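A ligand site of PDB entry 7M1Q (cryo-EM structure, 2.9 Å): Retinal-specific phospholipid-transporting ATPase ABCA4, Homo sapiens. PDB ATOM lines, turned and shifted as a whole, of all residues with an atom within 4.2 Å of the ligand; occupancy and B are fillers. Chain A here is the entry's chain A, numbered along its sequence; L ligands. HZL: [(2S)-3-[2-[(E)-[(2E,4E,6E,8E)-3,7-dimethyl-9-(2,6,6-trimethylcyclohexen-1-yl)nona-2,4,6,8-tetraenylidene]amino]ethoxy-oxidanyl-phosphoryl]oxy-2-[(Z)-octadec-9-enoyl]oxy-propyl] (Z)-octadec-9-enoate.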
ATOM      1  N   LEU A  42     -26.029  -5.747   7.724  1.00  0.00           N
ATOM      2  CA  LEU A  42     -24.889  -6.626   7.480  1.00  0.00           C
ATOM      3  C   LEU A  42     -24.463  -6.573   6.020  1.00  0.00           C
ATOM      4  O   LEU A  42     -23.269  -6.614   5.717  1.00  0.00           O
ATOM      5  CB  LEU A  42     -25.238  -8.053   7.890  1.00  0.00           C
ATOM      6  CG  LEU A  42     -25.129  -8.361   9.378  1.00  0.00           C
ATOM      7  CD1 LEU A  42     -25.976  -9.579   9.729  1.00  0.00           C
ATOM      8  CD2 LEU A  42     -23.682  -8.594   9.772  1.00  0.00           C
ATOM      9  N   ASN A  46     -20.728  -5.362   4.627  1.00  0.00           N
ATOM     10  CA  ASN A  46     -19.890  -6.352   3.957  1.00  0.00           C
ATOM     11  C   ASN A  46     -19.917  -6.083   2.460  1.00  0.00           C
ATOM     12  O   ASN A  46     -20.570  -6.799   1.690  1.00  0.00           O
ATOM     13  CB  ASN A  46     -20.350  -7.769   4.266  1.00  0.00           C
ATOM     14  CG  ASN A  46     -20.002  -8.193   5.676  1.00  0.00           C
ATOM     15  OD1 ASN A  46     -18.875  -8.583   5.960  1.00  0.00           O
ATOM     16  ND2 ASN A  46     -20.979  -8.130   6.565  1.00  0.00           N
ATOM     17  N   TRP A 339      -9.453 -14.090   7.628  1.00  0.00           N
ATOM     18  CA  TRP A 339      -8.780 -14.123   8.925  1.00  0.00           C
ATOM     19  C   TRP A 339      -9.208 -15.328   9.744  1.00  0.00           C
ATOM     20  O   TRP A 339      -8.408 -15.855  10.533  1.00  0.00           O
ATOM     21  CB  TRP A 339      -9.050 -12.841   9.695  1.00  0.00           C
ATOM     22  CG  TRP A 339     -10.507 -12.568   9.917  1.00  0.00           C
ATOM     23  CD1 TRP A 339     -11.320 -11.800   9.130  1.00  0.00           C
ATOM     24  CD2 TRP A 339     -11.331 -13.058  10.975  1.00  0.00           C
ATOM     25  NE1 TRP A 339     -12.593 -11.779   9.645  1.00  0.00           N
ATOM     26  CE2 TRP A 339     -12.626 -12.542  10.777  1.00  0.00           C
ATOM     27  CE3 TRP A 339     -11.090 -13.876  12.088  1.00  0.00           C
ATOM     28  CZ2 TRP A 339     -13.679 -12.831  11.635  1.00  0.00           C
ATOM     29  CZ3 TRP A 339     -12.140 -14.154  12.934  1.00  0.00           C
ATOM     30  CH2 TRP A 339     -13.419 -13.635  12.704  1.00  0.00           C
ATOM     31  N   TYR A 340     -10.446 -15.785   9.584  1.00  0.00           N
ATOM     32  CA  TYR A 340     -10.953 -16.908  10.365  1.00  0.00           C
ATOM     33  C   TYR A 340     -10.246 -18.214  10.043  1.00  0.00           C
ATOM     34  O   TYR A 340     -10.299 -19.147  10.850  1.00  0.00           O
ATOM     35  CB  TYR A 340     -12.453 -17.064  10.144  1.00  0.00           C
ATOM     36  CG  TYR A 340     -12.908 -16.755   8.736  1.00  0.00           C
ATOM     37  CD1 TYR A 340     -12.898 -17.738   7.758  1.00  0.00           C
ATOM     38  CD2 TYR A 340     -13.357 -15.495   8.391  1.00  0.00           C
ATOM     39  CE1 TYR A 340     -13.313 -17.470   6.478  1.00  0.00           C
ATOM     40  CE2 TYR A 340     -13.764 -15.216   7.106  1.00  0.00           C
ATOM     41  CZ  TYR A 340     -13.750 -16.200   6.159  1.00  0.00           C
ATOM     42  OH  TYR A 340     -14.165 -15.932   4.879  1.00  0.00           O
ATOM     43  N   TYR A 345      -8.322 -14.086  15.698  1.00  0.00           N
ATOM     44  CA  TYR A 345      -9.373 -13.272  16.304  1.00  0.00           C
ATOM     45  C   TYR A 345      -8.895 -11.860  16.584  1.00  0.00           C
ATOM     46  O   TYR A 345      -9.692 -10.914  16.588  1.00  0.00           O
ATOM     47  CB  TYR A 345      -9.876 -13.933  17.592  1.00  0.00           C
ATOM     48  CG  TYR A 345      -8.807 -14.135  18.638  1.00  0.00           C
ATOM     49  CD1 TYR A 345      -8.020 -15.274  18.643  1.00  0.00           C
ATOM     50  CD2 TYR A 345      -8.602 -13.195  19.640  1.00  0.00           C
ATOM     51  CE1 TYR A 345      -7.050 -15.463  19.594  1.00  0.00           C
ATOM     52  CE2 TYR A 345      -7.628 -13.375  20.599  1.00  0.00           C
ATOM     53  CZ  TYR A 345      -6.860 -14.515  20.570  1.00  0.00           C
ATOM     54  OH  TYR A 345      -5.894 -14.706  21.534  1.00  0.00           O
ATOM     55  N   PHE A 348      -9.622  -9.677  13.626  1.00  0.00           N
ATOM     56  CA  PHE A 348     -11.039  -9.304  13.564  1.00  0.00           C
ATOM     57  C   PHE A 348     -11.375  -8.234  14.578  1.00  0.00           C
ATOM     58  O   PHE A 348     -12.116  -7.288  14.281  1.00  0.00           O
ATOM     59  CB  PHE A 348     -11.914 -10.539  13.772  1.00  0.00           C
ATOM     60  CG  PHE A 348     -13.383 -10.231  13.853  1.00  0.00           C
ATOM     61  CD1 PHE A 348     -14.008  -9.528  12.843  1.00  0.00           C
ATOM     62  CD2 PHE A 348     -14.136 -10.642  14.939  1.00  0.00           C
ATOM     63  CE1 PHE A 348     -15.357  -9.244  12.906  1.00  0.00           C
ATOM     64  CE2 PHE A 348     -15.480 -10.357  15.011  1.00  0.00           C
ATOM     65  CZ  PHE A 348     -16.095  -9.664  13.996  1.00  0.00           C
ATOM     66  N   ARG A 587     -10.147 -24.376   3.895  1.00  0.00           N
ATOM     67  CA  ARG A 587     -11.516 -24.706   4.322  1.00  0.00           C
ATOM     68  C   ARG A 587     -12.545 -24.071   3.392  1.00  0.00           C
ATOM     69  O   ARG A 587     -12.681 -24.490   2.240  1.00  0.00           O
ATOM     70  CB  ARG A 587     -11.769 -24.261   5.758  1.00  0.00           C
ATOM     71  CG  ARG A 587     -12.892 -25.045   6.427  1.00  0.00           C
ATOM     72  CD  ARG A 587     -13.275 -24.482   7.783  1.00  0.00           C
ATOM     73  NE  ARG A 587     -14.526 -25.043   8.276  1.00  0.00           N
ATOM     74  CZ  ARG A 587     -15.688 -24.408   8.277  1.00  0.00           C
ATOM     75  NH1 ARG A 587     -15.798 -23.170   7.832  1.00  0.00           N
ATOM     76  NH2 ARG A 587     -16.764 -25.034   8.737  1.00  0.00           N
ATOM     77  N   TYR A 588     -13.262 -23.067   3.885  1.00  0.00           N
ATOM     78  CA  TYR A 588     -14.254 -22.391   3.059  1.00  0.00           C
ATOM     79  C   TYR A 588     -13.574 -21.752   1.859  1.00  0.00           C
ATOM     80  O   TYR A 588     -12.808 -20.800   2.008  1.00  0.00           O
ATOM     81  CB  TYR A 588     -15.002 -21.336   3.872  1.00  0.00           C
ATOM     82  CG  TYR A 588     -16.164 -20.726   3.115  1.00  0.00           C
ATOM     83  CD1 TYR A 588     -17.412 -21.324   3.110  1.00  0.00           C
ATOM     84  CD2 TYR A 588     -15.998 -19.540   2.401  1.00  0.00           C
ATOM     85  CE1 TYR A 588     -18.461 -20.773   2.419  1.00  0.00           C
ATOM     86  CE2 TYR A 588     -17.048 -18.979   1.710  1.00  0.00           C
ATOM     87  CZ  TYR A 588     -18.275 -19.595   1.717  1.00  0.00           C
ATOM     88  OH  TYR A 588     -19.325 -19.034   1.027  1.00  0.00           O
ATOM     89  N   ILE A 649     -21.628 -15.607   2.688  1.00  0.00           N
ATOM     90  CA  ILE A 649     -21.465 -16.517   3.822  1.00  0.00           C
ATOM     91  C   ILE A 649     -22.573 -16.295   4.834  1.00  0.00           C
ATOM     92  O   ILE A 649     -23.272 -17.224   5.247  1.00  0.00           O
ATOM     93  CB  ILE A 649     -20.073 -16.324   4.473  1.00  0.00           C
ATOM     94  CG1 ILE A 649     -18.959 -16.688   3.495  1.00  0.00           C
ATOM     95  CG2 ILE A 649     -19.969 -17.147   5.738  1.00  0.00           C
ATOM     96  CD1 ILE A 649     -17.582 -16.402   4.039  1.00  0.00           C
ATOM     97  N   ILE A 650     -22.791 -15.028   5.203  1.00  0.00           N
ATOM     98  CA  ILE A 650     -23.889 -14.699   6.094  1.00  0.00           C
ATOM     99  C   ILE A 650     -25.213 -15.127   5.480  1.00  0.00           C
ATOM    100  O   ILE A 650     -26.038 -15.780   6.124  1.00  0.00           O
ATOM    101  CB  ILE A 650     -23.883 -13.189   6.418  1.00  0.00           C
ATOM    102  CG1 ILE A 650     -22.823 -12.877   7.468  1.00  0.00           C
ATOM    103  CG2 ILE A 650     -25.255 -12.733   6.874  1.00  0.00           C
ATOM    104  CD1 ILE A 650     -22.262 -11.476   7.365  1.00  0.00           C
ATOM    105  N   ARG A 653     -25.964 -18.690   5.947  1.00  0.00           N
ATOM    106  CA  ARG A 653     -26.210 -19.168   7.299  1.00  0.00           C
ATOM    107  C   ARG A 653     -27.260 -18.372   8.052  1.00  0.00           C
ATOM    108  O   ARG A 653     -27.992 -18.949   8.849  1.00  0.00           O
ATOM    109  CB  ARG A 653     -24.901 -19.146   8.111  1.00  0.00           C
ATOM    110  CG  ARG A 653     -23.944 -20.266   7.754  1.00  0.00           C
ATOM    111  CD  ARG A 653     -24.330 -21.569   8.430  1.00  0.00           C
ATOM    112  NE  ARG A 653     -23.475 -22.680   8.014  1.00  0.00           N
ATOM    113  CZ  ARG A 653     -23.722 -23.441   6.962  1.00  0.00           C
ATOM    114  NH1 ARG A 653     -24.788 -23.252   6.198  1.00  0.00           N
ATOM    115  NH2 ARG A 653     -22.881 -24.427   6.664  1.00  0.00           N
ATOM    116  N   PHE A1397      -6.375 -27.113  19.083  1.00  0.00           N
ATOM    117  CA  PHE A1397      -5.984 -25.974  18.262  1.00  0.00           C
ATOM    118  C   PHE A1397      -4.481 -25.830  18.097  1.00  0.00           C
ATOM    119  O   PHE A1397      -4.041 -24.988  17.302  1.00  0.00           O
ATOM    120  CB  PHE A1397      -6.538 -24.681  18.865  1.00  0.00           C
ATOM    121  CG  PHE A1397      -8.027 -24.537  18.733  1.00  0.00           C
ATOM    122  CD1 PHE A1397      -8.875 -25.026  19.703  1.00  0.00           C
ATOM    123  CD2 PHE A1397      -8.575 -23.911  17.629  1.00  0.00           C
ATOM    124  CE1 PHE A1397     -10.239 -24.897  19.584  1.00  0.00           C
ATOM    125  CE2 PHE A1397      -9.937 -23.771  17.497  1.00  0.00           C
ATOM    126  CZ  PHE A1397     -10.779 -24.270  18.475  1.00  0.00           C
ATOM    127  N   PHE A1550     -16.476 -26.074   0.879  1.00  0.00           N
ATOM    128  CA  PHE A1550     -16.010 -26.269   2.255  1.00  0.00           C
ATOM    129  C   PHE A1550     -14.692 -27.009   2.344  1.00  0.00           C
ATOM    130  O   PHE A1550     -13.887 -26.713   3.234  1.00  0.00           O
ATOM    131  CB  PHE A1550     -17.079 -26.992   3.064  1.00  0.00           C
ATOM    132  CG  PHE A1550     -17.970 -26.065   3.831  1.00  0.00           C
ATOM    133  CD1 PHE A1550     -17.505 -25.378   4.927  1.00  0.00           C
ATOM    134  CD2 PHE A1550     -19.287 -25.865   3.437  1.00  0.00           C
ATOM    135  CE1 PHE A1550     -18.316 -24.518   5.631  1.00  0.00           C
ATOM    136  CE2 PHE A1550     -20.103 -25.005   4.132  1.00  0.00           C
ATOM    137  CZ  PHE A1550     -19.622 -24.327   5.231  1.00  0.00           C
ATOM    138  N   VAL A1673      -6.830 -19.039  24.584  1.00  0.00           N
ATOM    139  CA  VAL A1673      -8.021 -18.225  24.347  1.00  0.00           C
ATOM    140  C   VAL A1673      -9.042 -18.998  23.535  1.00  0.00           C
ATOM    141  O   VAL A1673     -10.236 -18.997  23.850  1.00  0.00           O
ATOM    142  CB  VAL A1673      -7.638 -16.901  23.650  1.00  0.00           C
ATOM    143  CG1 VAL A1673      -8.854 -16.273  23.012  1.00  0.00           C
ATOM    144  CG2 VAL A1673      -7.006 -15.955  24.640  1.00  0.00           C
ATOM    145  N   LEU A1674      -8.598 -19.698  22.490  1.00  0.00           N
ATOM    146  CA  LEU A1674      -9.536 -20.480  21.680  1.00  0.00           C
ATOM    147  C   LEU A1674     -10.158 -21.620  22.499  1.00  0.00           C
ATOM    148  O   LEU A1674     -11.377 -21.819  22.493  1.00  0.00           O
ATOM    149  CB  LEU A1674      -8.813 -21.035  20.450  1.00  0.00           C
ATOM    150  CG  LEU A1674      -8.282 -19.991  19.477  1.00  0.00           C
ATOM    151  CD1 LEU A1674      -7.312 -20.626  18.492  1.00  0.00           C
ATOM    152  CD2 LEU A1674      -9.421 -19.308  18.741  1.00  0.00           C
ATOM    153  N   SER A1677     -12.566 -20.271  24.920  1.00  0.00           N
ATOM    154  CA  SER A1677     -13.802 -19.837  24.274  1.00  0.00           C
ATOM    155  C   SER A1677     -14.743 -21.012  24.075  1.00  0.00           C
ATOM    156  O   SER A1677     -15.958 -20.898  24.296  1.00  0.00           O
ATOM    157  CB  SER A1677     -13.491 -19.160  22.951  1.00  0.00           C
ATOM    158  OG  SER A1677     -12.741 -20.022  22.110  1.00  0.00           O
ATOM    159  N   VAL A1678     -14.195 -22.152  23.653  1.00  0.00           N
ATOM    160  CA  VAL A1678     -15.012 -23.366  23.569  1.00  0.00           C
ATOM    161  C   VAL A1678     -15.591 -23.707  24.936  1.00  0.00           C
ATOM    162  O   VAL A1678     -16.781 -24.001  25.086  1.00  0.00           O
ATOM    163  CB  VAL A1678     -14.193 -24.533  22.981  1.00  0.00           C
ATOM    164  CG1 VAL A1678     -15.012 -25.813  23.002  1.00  0.00           C
ATOM    165  CG2 VAL A1678     -13.734 -24.206  21.577  1.00  0.00           C
ATOM    166  N   VAL A1681     -18.452 -21.369  25.854  1.00  0.00           N
ATOM    167  CA  VAL A1681     -19.705 -21.787  25.247  1.00  0.00           C
ATOM    168  C   VAL A1681     -20.300 -22.961  26.019  1.00  0.00           C
ATOM    169  O   VAL A1681     -21.513 -23.030  26.255  1.00  0.00           O
ATOM    170  CB  VAL A1681     -19.492 -22.134  23.762  1.00  0.00           C
ATOM    171  CG1 VAL A1681     -20.774 -22.678  23.152  1.00  0.00           C
ATOM    172  CG2 VAL A1681     -19.025 -20.917  23.000  1.00  0.00           C
ATOM    173  N   LEU A1815      -9.903  -9.831  26.340  1.00  0.00           N
ATOM    174  CA  LEU A1815      -8.957 -10.071  25.256  1.00  0.00           C
ATOM    175  C   LEU A1815      -8.196  -8.822  24.859  1.00  0.00           C
ATOM    176  O   LEU A1815      -7.066  -8.914  24.376  1.00  0.00           O
ATOM    177  CB  LEU A1815      -9.698 -10.636  24.043  1.00  0.00           C
ATOM    178  CG  LEU A1815     -10.362 -11.995  24.244  1.00  0.00           C
ATOM    179  CD1 LEU A1815     -11.111 -12.408  22.998  1.00  0.00           C
ATOM    180  CD2 LEU A1815      -9.328 -13.029  24.637  1.00  0.00           C
HETATM  181  CAK HZL L   1     -13.842 -14.309  19.054  1.00  0.00           C
HETATM  182  CAL HZL L   1     -13.008 -14.002  20.451  1.00  0.00           C
HETATM  183  CAM HZL L   1     -11.936 -14.819  20.615  1.00  0.00           C
HETATM  184  CAN HZL L   1     -13.719 -15.663  18.545  1.00  0.00           C
HETATM  185  CAO HZL L   1     -12.421 -16.391  20.704  1.00  0.00           C
HETATM  186  CAP HZL L   1     -13.147 -16.794  19.524  1.00  0.00           C
HETATM  187  CAQ HZL L   1     -15.331 -14.053  19.339  1.00  0.00           C
HETATM  188  CAR HZL L   1     -13.374 -13.318  17.947  1.00  0.00           C
HETATM  189  CAS HZL L   1     -14.717 -16.084  17.408  1.00  0.00           C
HETATM  190  CAT HZL L   1     -13.747 -18.203  19.467  1.00  0.00           C
HETATM  191  CAU HZL L   1     -14.417 -16.768  16.246  1.00  0.00           C
HETATM  192  CAV HZL L   1     -13.041 -17.330  15.723  1.00  0.00           C
HETATM  193  CAW HZL L   1     -11.735 -17.349  16.560  1.00  0.00           C
HETATM  194  CAX HZL L   1     -13.016 -17.833  14.443  1.00  0.00           C
HETATM  195  CAY HZL L   1     -17.699 -10.873   9.000  1.00  0.00           C
HETATM  196  CAZ HZL L   1     -18.278 -11.465  10.338  1.00  0.00           C
HETATM  197  CBA HZL L   1     -12.814 -24.630  14.207  1.00  0.00           C
HETATM  198  CBB HZL L   1     -13.048 -26.027  13.616  1.00  0.00           C
HETATM  199  CBC HZL L   1     -16.915 -11.963   8.157  1.00  0.00           C
HETATM  200  CBD HZL L   1     -19.381 -10.909  10.898  1.00  0.00           C
HETATM  201  CBE HZL L   1     -13.288 -24.333  15.380  1.00  0.00           C
HETATM  202  CBF HZL L   1     -14.411 -26.142  12.914  1.00  0.00           C
HETATM  203  CBG HZL L   1     -17.708 -13.314   8.053  1.00  0.00           C
HETATM  204  CBH HZL L   1     -14.842 -24.795  12.263  1.00  0.00           C
HETATM  205  CBI HZL L   1     -17.005 -14.488   8.794  1.00  0.00           C
HETATM  206  CBJ HZL L   1     -16.345 -24.487  12.474  1.00  0.00           C
HETATM  207  CBK HZL L   1     -17.883 -15.100   9.929  1.00  0.00           C
HETATM  208  CBL HZL L   1     -16.608 -22.991  12.783  1.00  0.00           C
HETATM  209  CBM HZL L   1     -14.358 -17.780  13.658  1.00  0.00           C
HETATM  210  CBN HZL L   1     -19.401 -15.150   9.556  1.00  0.00           C
HETATM  211  CBO HZL L   1     -18.000 -22.760  13.436  1.00  0.00           C
HETATM  212  CBP HZL L   1     -19.937 -16.608   9.432  1.00  0.00           C
HETATM  213  CBQ HZL L   1     -17.978 -21.625  14.496  1.00  0.00           C
HETATM  214  CBR HZL L   1     -14.571 -18.503  12.531  1.00  0.00           C
HETATM  215  CBS HZL L   1     -21.219 -16.845  10.263  1.00  0.00           C
HETATM  216  CBT HZL L   1     -18.676 -20.320  13.976  1.00  0.00           C
HETATM  217  CBU HZL L   1     -20.381 -18.931  11.010  1.00  0.00           C
HETATM  218  CBV HZL L   1     -15.947 -18.339  11.864  1.00  0.00           C
HETATM  219  CBW HZL L   1     -20.288 -19.291  12.497  1.00  0.00           C
HETATM  220  CBX HZL L   1     -20.507 -20.231  10.178  1.00  0.00           C
HETATM  221  CBY HZL L   1     -17.033 -17.484  12.566  1.00  0.00           C
HETATM  222  CBZ HZL L   1     -16.231 -18.916  10.669  1.00  0.00           C
HETATM  223  CCA HZL L   1     -15.179 -19.793   9.917  1.00  0.00           C
HETATM  224  CCB HZL L   1     -16.404 -19.214   7.916  1.00  0.00           C
HETATM  225  CCC HZL L   1     -17.035 -20.155   6.822  1.00  0.00           C
HETATM  226  CCD HZL L   1     -13.052 -22.947  15.970  1.00  0.00           C
HETATM  227  CCE HZL L   1     -14.343 -22.313  16.503  1.00  0.00           C
HETATM  228  CCF HZL L   1     -20.081  -9.687  10.222  1.00  0.00           C
HETATM  229  CCG HZL L   1     -19.879  -8.386  11.024  1.00  0.00           C
HETATM  230  CCH HZL L   1     -18.640  -7.596  10.554  1.00  0.00           C
HETATM  231  CCI HZL L   1     -18.835  -6.062  10.679  1.00  0.00           C
HETATM  232  CCJ HZL L   1     -17.883  -5.411  11.734  1.00  0.00           C
HETATM  233  CCK HZL L   1     -18.659  -4.864  12.970  1.00  0.00           C
HETATM  234  CCL HZL L   1     -19.308  -5.997  13.803  1.00  0.00           C
HETATM  235  CCM HZL L   1     -19.377  -5.642  15.302  1.00  0.00           C
HETATM  236  CCN HZL L   1     -14.118 -21.608  17.839  1.00  0.00           C
HETATM  237  CCO HZL L   1     -15.355 -21.630  18.732  1.00  0.00           C
HETATM  238  CCP HZL L   1     -16.421 -20.638  18.266  1.00  0.00           C
HETATM  239  CCQ HZL L   1     -17.191 -20.045  19.419  1.00  0.00           C
HETATM  240  CCR HZL L   1     -18.405 -19.264  18.957  1.00  0.00           C
HETATM  241  CCS HZL L   1     -18.067 -17.812  18.643  1.00  0.00           C
HETATM  242  NAJ HZL L   1     -15.286 -19.909   8.630  1.00  0.00           N
HETATM  243  OAB HZL L   1     -21.501 -18.139  10.793  1.00  0.00           O
HETATM  244  OAC HZL L   1     -19.276 -20.297  12.663  1.00  0.00           O
HETATM  245  OAD HZL L   1     -21.965 -15.943  10.479  1.00  0.00           O
HETATM  246  OAE HZL L   1     -18.713 -19.347  14.663  1.00  0.00           O
HETATM  247  OAF HZL L   1     -19.257 -20.504   9.591  1.00  0.00           O
HETATM  248  OAG HZL L   1     -18.481 -20.118   6.953  1.00  0.00           O
HETATM  249  OAH HZL L   1     -20.639 -21.471   7.594  1.00  0.00           O
HETATM  250  OAI HZL L   1     -18.444 -22.498   8.086  1.00  0.00           O
HETATM  251  PAA HZL L   1     -19.231 -21.196   8.042  1.00  0.00           P
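Residues that only touch the ligand: Phe 1550 (3.2 Å), Tyr 340 (3.3 Å), Ser 1677 (3.4 Å), Leu 1815 (3.5 Å), Ile 649 (3.5 Å), Phe 1397 (3.6 Å), Tyr 345 (3.6 Å), Leu 1674 (3.7 Å), Tyr 588 (3.8 Å), Leu 42 (3.8 Å) and Asn 46 (3.98 Å).
13 residues have an atom within 4 Å of the ligand: Leu 42, Asn 46, Tyr 340, Tyr 345, Arg 587, Tyr 588, Ile 649, Arg 653, Phe 1397, Phe 1550, Leu 1674, Ser 1677 and Leu 1815.
The nearest printed residue that does not touch the ligand is Ile 650 (4.01 Å).
The backbone carbonyl oxygen (O) of Leu 42 lies within hydrogen-bond range of the side-chain amide nitrogen (ND2) of Asn 46 (2.9 Å).
The backbone carbonyl oxygen of Phe 1550 lies close to the backbone carbonyl oxygen of Arg 587, 2.7 Å away.
OG of Ser 1677 sits at hydrogen-bond distance from O of Val 1673, 3.2 Å away.
NE of Arg 653 is in salt-bridge range of OAH of the ligand, at 3.1 Å.
OAI of the ligand is in salt-bridge range of NH1 of Arg 587 (2.7 Å).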
